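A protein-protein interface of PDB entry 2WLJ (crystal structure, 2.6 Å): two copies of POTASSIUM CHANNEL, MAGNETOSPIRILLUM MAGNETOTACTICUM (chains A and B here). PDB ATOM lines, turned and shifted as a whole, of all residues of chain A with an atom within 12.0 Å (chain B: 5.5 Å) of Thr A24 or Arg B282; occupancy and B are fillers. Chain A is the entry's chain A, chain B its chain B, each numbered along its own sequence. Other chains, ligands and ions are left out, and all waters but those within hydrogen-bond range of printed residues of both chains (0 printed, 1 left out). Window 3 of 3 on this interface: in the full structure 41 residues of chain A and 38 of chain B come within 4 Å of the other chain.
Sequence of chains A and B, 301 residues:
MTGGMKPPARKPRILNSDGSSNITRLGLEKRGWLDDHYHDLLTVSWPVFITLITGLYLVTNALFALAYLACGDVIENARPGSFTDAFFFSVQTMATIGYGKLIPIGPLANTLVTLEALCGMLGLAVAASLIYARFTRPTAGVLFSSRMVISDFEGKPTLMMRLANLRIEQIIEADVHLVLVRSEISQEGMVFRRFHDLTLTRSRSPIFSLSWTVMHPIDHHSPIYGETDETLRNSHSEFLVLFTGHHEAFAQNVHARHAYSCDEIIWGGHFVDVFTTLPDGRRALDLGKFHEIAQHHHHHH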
ATOM      1  N   PRO A  12      -1.817 -11.164  -1.496  1.00  0.00           N
ATOM      2  CA  PRO A  12      -2.309 -11.706  -0.239  1.00  0.00           C
ATOM      3  C   PRO A  12      -3.331 -10.822   0.457  1.00  0.00           C
ATOM      4  O   PRO A  12      -3.942 -11.277   1.415  1.00  0.00           O
ATOM      5  CB  PRO A  12      -1.041 -11.799   0.617  1.00  0.00           C
ATOM      6  CG  PRO A  12       0.034 -12.133  -0.375  1.00  0.00           C
ATOM      7  CD  PRO A  12      -0.358 -11.382  -1.648  1.00  0.00           C
ATOM      8  N   ARG A  13      -3.531  -9.589  -0.002  1.00  0.00           N
ATOM      9  CA  ARG A  13      -4.445  -8.655   0.693  1.00  0.00           C
ATOM     10  C   ARG A  13      -5.834  -8.590   0.093  1.00  0.00           C
ATOM     11  O   ARG A  13      -5.977  -8.269  -1.086  1.00  0.00           O
ATOM     12  CB  ARG A  13      -3.885  -7.242   0.660  1.00  0.00           C
ATOM     13  CG  ARG A  13      -3.290  -6.767   1.942  1.00  0.00           C
ATOM     14  CD  ARG A  13      -3.272  -5.276   1.886  1.00  0.00           C
ATOM     15  NE  ARG A  13      -2.289  -4.732   2.811  1.00  0.00           N
ATOM     16  CZ  ARG A  13      -2.580  -4.267   4.018  1.00  0.00           C
ATOM     17  NH1 ARG A  13      -3.838  -4.281   4.452  1.00  0.00           N
ATOM     18  NH2 ARG A  13      -1.609  -3.784   4.783  1.00  0.00           N
ATOM     19  N   ILE A  14      -6.865  -8.852   0.886  1.00  0.00           N
ATOM     20  CA  ILE A  14      -8.216  -8.766   0.334  1.00  0.00           C
ATOM     21  C   ILE A  14      -8.738  -7.314   0.310  1.00  0.00           C
ATOM     22  O   ILE A  14      -9.315  -6.872  -0.688  1.00  0.00           O
ATOM     23  CB  ILE A  14      -9.184  -9.747   1.035  1.00  0.00           C
ATOM     24  CG1 ILE A  14      -8.693 -11.194   0.829  1.00  0.00           C
ATOM     25  CG2 ILE A  14     -10.630  -9.555   0.537  1.00  0.00           C
ATOM     26  CD1 ILE A  14      -9.375 -12.233   1.732  1.00  0.00           C
ATOM     27  N   LEU A  15      -8.520  -6.578   1.399  1.00  0.00           N
ATOM     28  CA  LEU A  15      -8.741  -5.148   1.425  1.00  0.00           C
ATOM     29  C   LEU A  15      -7.385  -4.468   1.421  1.00  0.00           C
ATOM     30  O   LEU A  15      -6.459  -4.914   2.092  1.00  0.00           O
ATOM     31  CB  LEU A  15      -9.521  -4.747   2.683  1.00  0.00           C
ATOM     32  CG  LEU A  15     -10.922  -5.378   2.755  1.00  0.00           C
ATOM     33  CD1 LEU A  15     -11.343  -5.662   4.197  1.00  0.00           C
ATOM     34  CD2 LEU A  15     -12.013  -4.596   1.970  1.00  0.00           C
ATOM     35  N   ASN A  16      -7.256  -3.400   0.644  1.00  0.00           N
ATOM     36  CA  ASN A  16      -6.094  -2.546   0.775  1.00  0.00           C
ATOM     37  C   ASN A  16      -6.253  -1.603   1.959  1.00  0.00           C
ATOM     38  O   ASN A  16      -7.362  -1.341   2.418  1.00  0.00           O
ATOM     39  CB  ASN A  16      -5.960  -1.604  -0.434  1.00  0.00           C
ATOM     40  CG  ASN A  16      -6.054  -2.342  -1.784  1.00  0.00           C
ATOM     41  OD1 ASN A  16      -5.193  -3.156  -2.120  1.00  0.00           O
ATOM     42  ND2 ASN A  16      -7.080  -2.036  -2.555  1.00  0.00           N
ATOM     43  N   SER A  20     -10.216  -0.084   0.222  1.00  0.00           N
ATOM     44  CA  SER A  20     -10.762  -0.496  -1.068  1.00  0.00           C
ATOM     45  C   SER A  20     -10.409  -1.948  -1.379  1.00  0.00           C
ATOM     46  O   SER A  20      -9.447  -2.512  -0.840  1.00  0.00           O
ATOM     47  CB  SER A  20     -10.226   0.384  -2.187  1.00  0.00           C
ATOM     48  OG  SER A  20      -8.816   0.268  -2.245  1.00  0.00           O
ATOM     49  N   SER A  21     -11.185  -2.530  -2.282  1.00  0.00           N
ATOM     50  CA  SER A  21     -11.072  -3.943  -2.604  1.00  0.00           C
ATOM     51  C   SER A  21      -9.863  -4.272  -3.449  1.00  0.00           C
ATOM     52  O   SER A  21      -9.494  -3.541  -4.360  1.00  0.00           O
ATOM     53  CB  SER A  21     -12.316  -4.451  -3.334  1.00  0.00           C
ATOM     54  OG  SER A  21     -12.198  -5.861  -3.493  1.00  0.00           O
ATOM     55  N   ASN A  22      -9.262  -5.406  -3.171  1.00  0.00           N
ATOM     56  CA  ASN A  22      -8.116  -5.775  -3.953  1.00  0.00           C
ATOM     57  C   ASN A  22      -8.455  -6.753  -5.051  1.00  0.00           C
ATOM     58  O   ASN A  22      -7.612  -7.055  -5.855  1.00  0.00           O
ATOM     59  CB  ASN A  22      -7.045  -6.386  -3.074  1.00  0.00           C
ATOM     60  CG  ASN A  22      -5.675  -6.244  -3.668  1.00  0.00           C
ATOM     61  OD1 ASN A  22      -5.480  -5.493  -4.626  1.00  0.00           O
ATOM     62  ND2 ASN A  22      -4.708  -6.939  -3.084  1.00  0.00           N
ATOM     63  N   ILE A  23      -9.684  -7.238  -5.087  1.00  0.00           N
ATOM     64  CA  ILE A  23     -10.111  -8.203  -6.087  1.00  0.00           C
ATOM     65  C   ILE A  23     -10.117  -7.649  -7.522  1.00  0.00           C
ATOM     66  O   ILE A  23     -10.202  -6.441  -7.735  1.00  0.00           O
ATOM     67  CB  ILE A  23     -11.499  -8.769  -5.727  1.00  0.00           C
ATOM     68  CG1 ILE A  23     -11.375  -9.800  -4.591  1.00  0.00           C
ATOM     69  CG2 ILE A  23     -12.132  -9.424  -6.919  1.00  0.00           C
ATOM     70  CD1 ILE A  23     -10.854  -9.243  -3.251  1.00  0.00           C
ATOM     71  N   THR A  24     -10.001  -8.548  -8.500  1.00  0.00           N
ATOM     72  CA  THR A  24     -10.086  -8.190  -9.912  1.00  0.00           C
ATOM     73  C   THR A  24     -11.527  -8.362 -10.342  1.00  0.00           C
ATOM     74  O   THR A  24     -12.190  -9.326  -9.939  1.00  0.00           O
ATOM     75  CB  THR A  24      -9.194  -9.109 -10.779  1.00  0.00           C
ATOM     76  OG1 THR A  24      -7.810  -8.833 -10.518  1.00  0.00           O
ATOM     77  CG2 THR A  24      -9.466  -8.891 -12.253  1.00  0.00           C
ATOM     78  N   ARG A  25     -12.015  -7.444 -11.166  1.00  0.00           N
ATOM     79  CA  ARG A  25     -13.426  -7.430 -11.535  1.00  0.00           C
ATOM     80  C   ARG A  25     -13.683  -7.854 -12.981  1.00  0.00           C
ATOM     81  O   ARG A  25     -13.175  -7.236 -13.923  1.00  0.00           O
ATOM     82  CB  ARG A  25     -14.032  -6.048 -11.271  1.00  0.00           C
ATOM     83  CG  ARG A  25     -14.402  -5.811  -9.821  1.00  0.00           C
ATOM     84  CD  ARG A  25     -14.602  -4.334  -9.529  1.00  0.00           C
ATOM     85  NE  ARG A  25     -13.346  -3.666  -9.201  1.00  0.00           N
ATOM     86  CZ  ARG A  25     -12.995  -3.318  -7.970  1.00  0.00           C
ATOM     87  NH1 ARG A  25     -13.808  -3.570  -6.961  1.00  0.00           N
ATOM     88  NH2 ARG A  25     -11.839  -2.714  -7.755  1.00  0.00           N
ATOM     89  N   LEU A  26     -14.476  -8.904 -13.155  1.00  0.00           N
ATOM     90  CA  LEU A  26     -14.864  -9.372 -14.478  1.00  0.00           C
ATOM     91  C   LEU A  26     -16.383  -9.236 -14.552  1.00  0.00           C
ATOM     92  O   LEU A  26     -17.080  -9.422 -13.544  1.00  0.00           O
ATOM     93  CB  LEU A  26     -14.464 -10.843 -14.664  1.00  0.00           C
ATOM     94  CG  LEU A  26     -13.006 -11.307 -14.784  1.00  0.00           C
ATOM     95  CD1 LEU A  26     -12.024 -10.280 -14.262  1.00  0.00           C
ATOM     96  CD2 LEU A  26     -12.816 -12.626 -14.050  1.00  0.00           C
ATOM     97  N   GLY A  27     -16.901  -8.901 -15.731  1.00  0.00           N
ATOM     98  CA  GLY A  27     -18.356  -8.837 -15.927  1.00  0.00           C
ATOM     99  C   GLY A  27     -18.842  -7.567 -16.609  1.00  0.00           C
ATOM    100  O   GLY A  27     -19.531  -6.744 -15.989  1.00  0.00           O
ATOM    101  N   HIS A 236      -7.364 -15.827   7.392  1.00  0.00           N
ATOM    102  CA  HIS A 236      -7.243 -14.719   6.459  1.00  0.00           C
ATOM    103  C   HIS A 236      -7.969 -13.484   7.012  1.00  0.00           C
ATOM    104  O   HIS A 236      -8.651 -12.783   6.273  1.00  0.00           O
ATOM    105  CB  HIS A 236      -7.809 -15.123   5.089  1.00  0.00           C
ATOM    106  CG  HIS A 236      -7.033 -16.219   4.407  1.00  0.00           C
ATOM    107  ND1 HIS A 236      -5.868 -15.985   3.703  1.00  0.00           N
ATOM    108  CD2 HIS A 236      -7.261 -17.554   4.315  1.00  0.00           C
ATOM    109  CE1 HIS A 236      -5.411 -17.127   3.212  1.00  0.00           C
ATOM    110  NE2 HIS A 236      -6.239 -18.093   3.567  1.00  0.00           N
ATOM    111  N   THR B 276     -13.604 -16.133  -7.398  1.00  0.00           N
ATOM    112  CA  THR B 276     -12.851 -17.209  -7.994  1.00  0.00           C
ATOM    113  C   THR B 276     -11.397 -16.838  -7.987  1.00  0.00           C
ATOM    114  O   THR B 276     -11.066 -15.665  -7.914  1.00  0.00           O
ATOM    115  CB  THR B 276     -13.304 -17.424  -9.446  1.00  0.00           C
ATOM    116  OG1 THR B 276     -13.116 -16.208 -10.182  1.00  0.00           O
ATOM    117  CG2 THR B 276     -14.800 -17.803  -9.505  1.00  0.00           C
ATOM    118  N   THR B 277     -10.520 -17.835  -8.065  1.00  0.00           N
ATOM    119  CA  THR B 277      -9.086 -17.553  -8.216  1.00  0.00           C
ATOM    120  C   THR B 277      -8.624 -17.560  -9.676  1.00  0.00           C
ATOM    121  O   THR B 277      -9.029 -18.419 -10.453  1.00  0.00           O
ATOM    122  CB  THR B 277      -8.230 -18.516  -7.393  1.00  0.00           C
ATOM    123  OG1 THR B 277      -8.503 -18.291  -6.008  1.00  0.00           O
ATOM    124  CG2 THR B 277      -6.745 -18.280  -7.651  1.00  0.00           C
ATOM    125  N   LEU B 278      -7.785 -16.594 -10.042  1.00  0.00           N
ATOM    126  CA  LEU B 278      -7.308 -16.483 -11.413  1.00  0.00           C
ATOM    127  C   LEU B 278      -6.119 -17.396 -11.720  1.00  0.00           C
ATOM    128  O   LEU B 278      -5.648 -18.150 -10.852  1.00  0.00           O
ATOM    129  CB  LEU B 278      -6.953 -15.038 -11.753  1.00  0.00           C
ATOM    130  CG  LEU B 278      -8.183 -14.215 -12.092  1.00  0.00           C
ATOM    131  CD1 LEU B 278      -7.837 -13.030 -12.991  1.00  0.00           C
ATOM    132  CD2 LEU B 278      -9.198 -15.126 -12.765  1.00  0.00           C
ATOM    133  N   PRO B 279      -5.638 -17.336 -12.977  1.00  0.00           N
ATOM    134  CA  PRO B 279      -4.438 -18.063 -13.376  1.00  0.00           C
ATOM    135  C   PRO B 279      -3.301 -17.776 -12.387  1.00  0.00           C
ATOM    136  O   PRO B 279      -2.703 -18.706 -11.839  1.00  0.00           O
ATOM    137  CB  PRO B 279      -4.108 -17.468 -14.758  1.00  0.00           C
ATOM    138  CG  PRO B 279      -5.408 -16.916 -15.271  1.00  0.00           C
ATOM    139  CD  PRO B 279      -6.158 -16.464 -14.052  1.00  0.00           C
ATOM    140  N   ASP B 280      -3.038 -16.486 -12.152  1.00  0.00           N
ATOM    141  CA  ASP B 280      -1.951 -16.043 -11.270  1.00  0.00           C
ATOM    142  C   ASP B 280      -2.177 -16.431  -9.798  1.00  0.00           C
ATOM    143  O   ASP B 280      -1.229 -16.667  -9.050  1.00  0.00           O
ATOM    144  CB  ASP B 280      -1.764 -14.519 -11.368  1.00  0.00           C
ATOM    145  CG  ASP B 280      -2.301 -13.937 -12.667  1.00  0.00           C
ATOM    146  OD1 ASP B 280      -2.904 -14.689 -13.467  1.00  0.00           O
ATOM    147  OD2 ASP B 280      -2.125 -12.719 -12.885  1.00  0.00           O
ATOM    148  N   GLY B 281      -3.434 -16.493  -9.383  1.00  0.00           N
ATOM    149  CA  GLY B 281      -3.755 -16.621  -7.960  1.00  0.00           C
ATOM    150  C   GLY B 281      -4.325 -15.307  -7.433  1.00  0.00           C
ATOM    151  O   GLY B 281      -4.501 -15.129  -6.233  1.00  0.00           O
ATOM    152  N   ARG B 282      -4.577 -14.375  -8.348  1.00  0.00           N
ATOM    153  CA  ARG B 282      -5.318 -13.175  -8.038  1.00  0.00           C
ATOM    154  C   ARG B 282      -6.740 -13.594  -7.732  1.00  0.00           C
ATOM    155  O   ARG B 282      -7.266 -14.525  -8.360  1.00  0.00           O
ATOM    156  CB  ARG B 282      -5.356 -12.248  -9.245  1.00  0.00           C
ATOM    157  CG  ARG B 282      -4.143 -11.395  -9.435  1.00  0.00           C
ATOM    158  CD  ARG B 282      -4.383 -10.498 -10.624  1.00  0.00           C
ATOM    159  NE  ARG B 282      -4.374 -11.255 -11.876  1.00  0.00           N
ATOM    160  CZ  ARG B 282      -4.812 -10.793 -13.047  1.00  0.00           C
ATOM    161  NH1 ARG B 282      -5.323  -9.568 -13.140  1.00  0.00           N
ATOM    162  NH2 ARG B 282      -4.746 -11.560 -14.130  1.00  0.00           N
ATOM    163  N   ARG B 283      -7.369 -12.910  -6.777  1.00  0.00           N
ATOM    164  CA  ARG B 283      -8.779 -13.124  -6.529  1.00  0.00           C
ATOM    165  C   ARG B 283      -9.584 -12.340  -7.576  1.00  0.00           C
ATOM    166  O   ARG B 283      -9.197 -11.244  -8.002  1.00  0.00           O
ATOM    167  CB  ARG B 283      -9.153 -12.733  -5.091  1.00  0.00           C
ATOM    168  CG  ARG B 283     -10.453 -13.393  -4.570  1.00  0.00           C
ATOM    169  CD  ARG B 283     -10.299 -14.921  -4.317  1.00  0.00           C
ATOM    170  NE  ARG B 283     -11.587 -15.641  -4.342  1.00  0.00           N
ATOM    171  CZ  ARG B 283     -11.768 -16.903  -3.933  1.00  0.00           C
ATOM    172  NH1 ARG B 283     -10.747 -17.602  -3.452  1.00  0.00           N
ATOM    173  NH2 ARG B 283     -12.969 -17.473  -3.993  1.00  0.00           N
ATOM    174  N   ALA B 284     -10.688 -12.920  -8.025  1.00  0.00           N
ATOM    175  CA  ALA B 284     -11.486 -12.276  -9.051  1.00  0.00           C
ATOM    176  C   ALA B 284     -12.951 -12.368  -8.692  1.00  0.00           C
ATOM    177  O   ALA B 284     -13.374 -13.295  -8.016  1.00  0.00           O
ATOM    178  CB  ALA B 284     -11.225 -12.917 -10.414  1.00  0.00           C
ATOM    179  N   LEU B 285     -13.725 -11.392  -9.141  1.00  0.00           N
ATOM    180  CA  LEU B 285     -15.175 -11.504  -9.042  1.00  0.00           C
ATOM    181  C   LEU B 285     -15.769 -11.673 -10.429  1.00  0.00           C
ATOM    182  O   LEU B 285     -15.547 -10.869 -11.319  1.00  0.00           O
ATOM    183  CB  LEU B 285     -15.786 -10.281  -8.345  1.00  0.00           C
ATOM    184  CG  LEU B 285     -17.314 -10.188  -8.384  1.00  0.00           C
ATOM    185  CD1 LEU B 285     -17.915 -11.243  -7.469  1.00  0.00           C
ATOM    186  CD2 LEU B 285     -17.816  -8.781  -8.027  1.00  0.00           C
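O of Thr A24 is in hydrogen-bond range of N of Leu B285 (2.7 Å). N of Thr A24 is in hydrogen-bond range of O of Arg B283, at 2.9 Å. The backbone NH (N) of Leu A26 sits at hydrogen-bond distance from the backbone carbonyl oxygen (O) of Leu B285 (2.9 Å).
The backbone carbonyl oxygen (O) of Thr B276 is in hydrogen-bond range of the backbone NH (N) of Ala B284. NH1 of Arg B283 is in hydrogen-bond range of OG1 of Thr B277, at 3.5 Å. OG of Ser A21 is in hydrogen-bond range of N of Ile A23. The side-chain carboxylate (OD2) of Asp B280 lies within salt-bridge range of the guanidinium group (NE) of Arg B282, at 2.9 Å.
Arg B283 touches Ile A23 (O to CG2, 3.6 Å). Ile A23 touches Ala B284 (CG2 to C, 3.5 Å). Ile A23 touches Leu B285 (CG2 to N, 3.4 Å). Arg B282 touches Thr A24 (NH1 to OG1, 3.7 Å). Ala B284 touches Thr A24. Leu B285 touches Arg A25 (O to C, 3.9 Å). Leu A26 touches Ala B284 (CD2 to CB, 3.98 Å).
Asn A16 touches none of the printed residues of chain B. Of the printed residues of chain B, Ile A23 touches Arg B283, Ala B284 and Leu B285. Of chain B, only Arg B282 (3.7 Å), Arg B283 (2.9 Å), Ala B284 (3.2 Å) and Leu B285 (2.7 Å) come within 4 Å of Thr A24. Of the printed residues of chain B, Arg A25 touches Leu B285. Printed residues of chain B within 4 Å of Leu A26: Ala B284 and Leu B285. No residue of chain A comes within 4 Å of Asp B280. Arg B282 touches just one residue of chain A: Thr A24 (3.7 Å). Ala B284 touches three residues of chain A. Of the printed residues of chain A, Leu B285 touches Ile A23, Thr A24, Arg A25 and Leu A26. The nearest printed residue of chain B that does not touch Ile A23 is Thr B276 (6.4 Å).
Hydrophobic or aromatic side chains of chain A within 4 Å of the printed part of chain B: Ile A23 and Leu A26. Among the printed residues, 10 pairs touch across the chains.
No position is printed for both chains.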
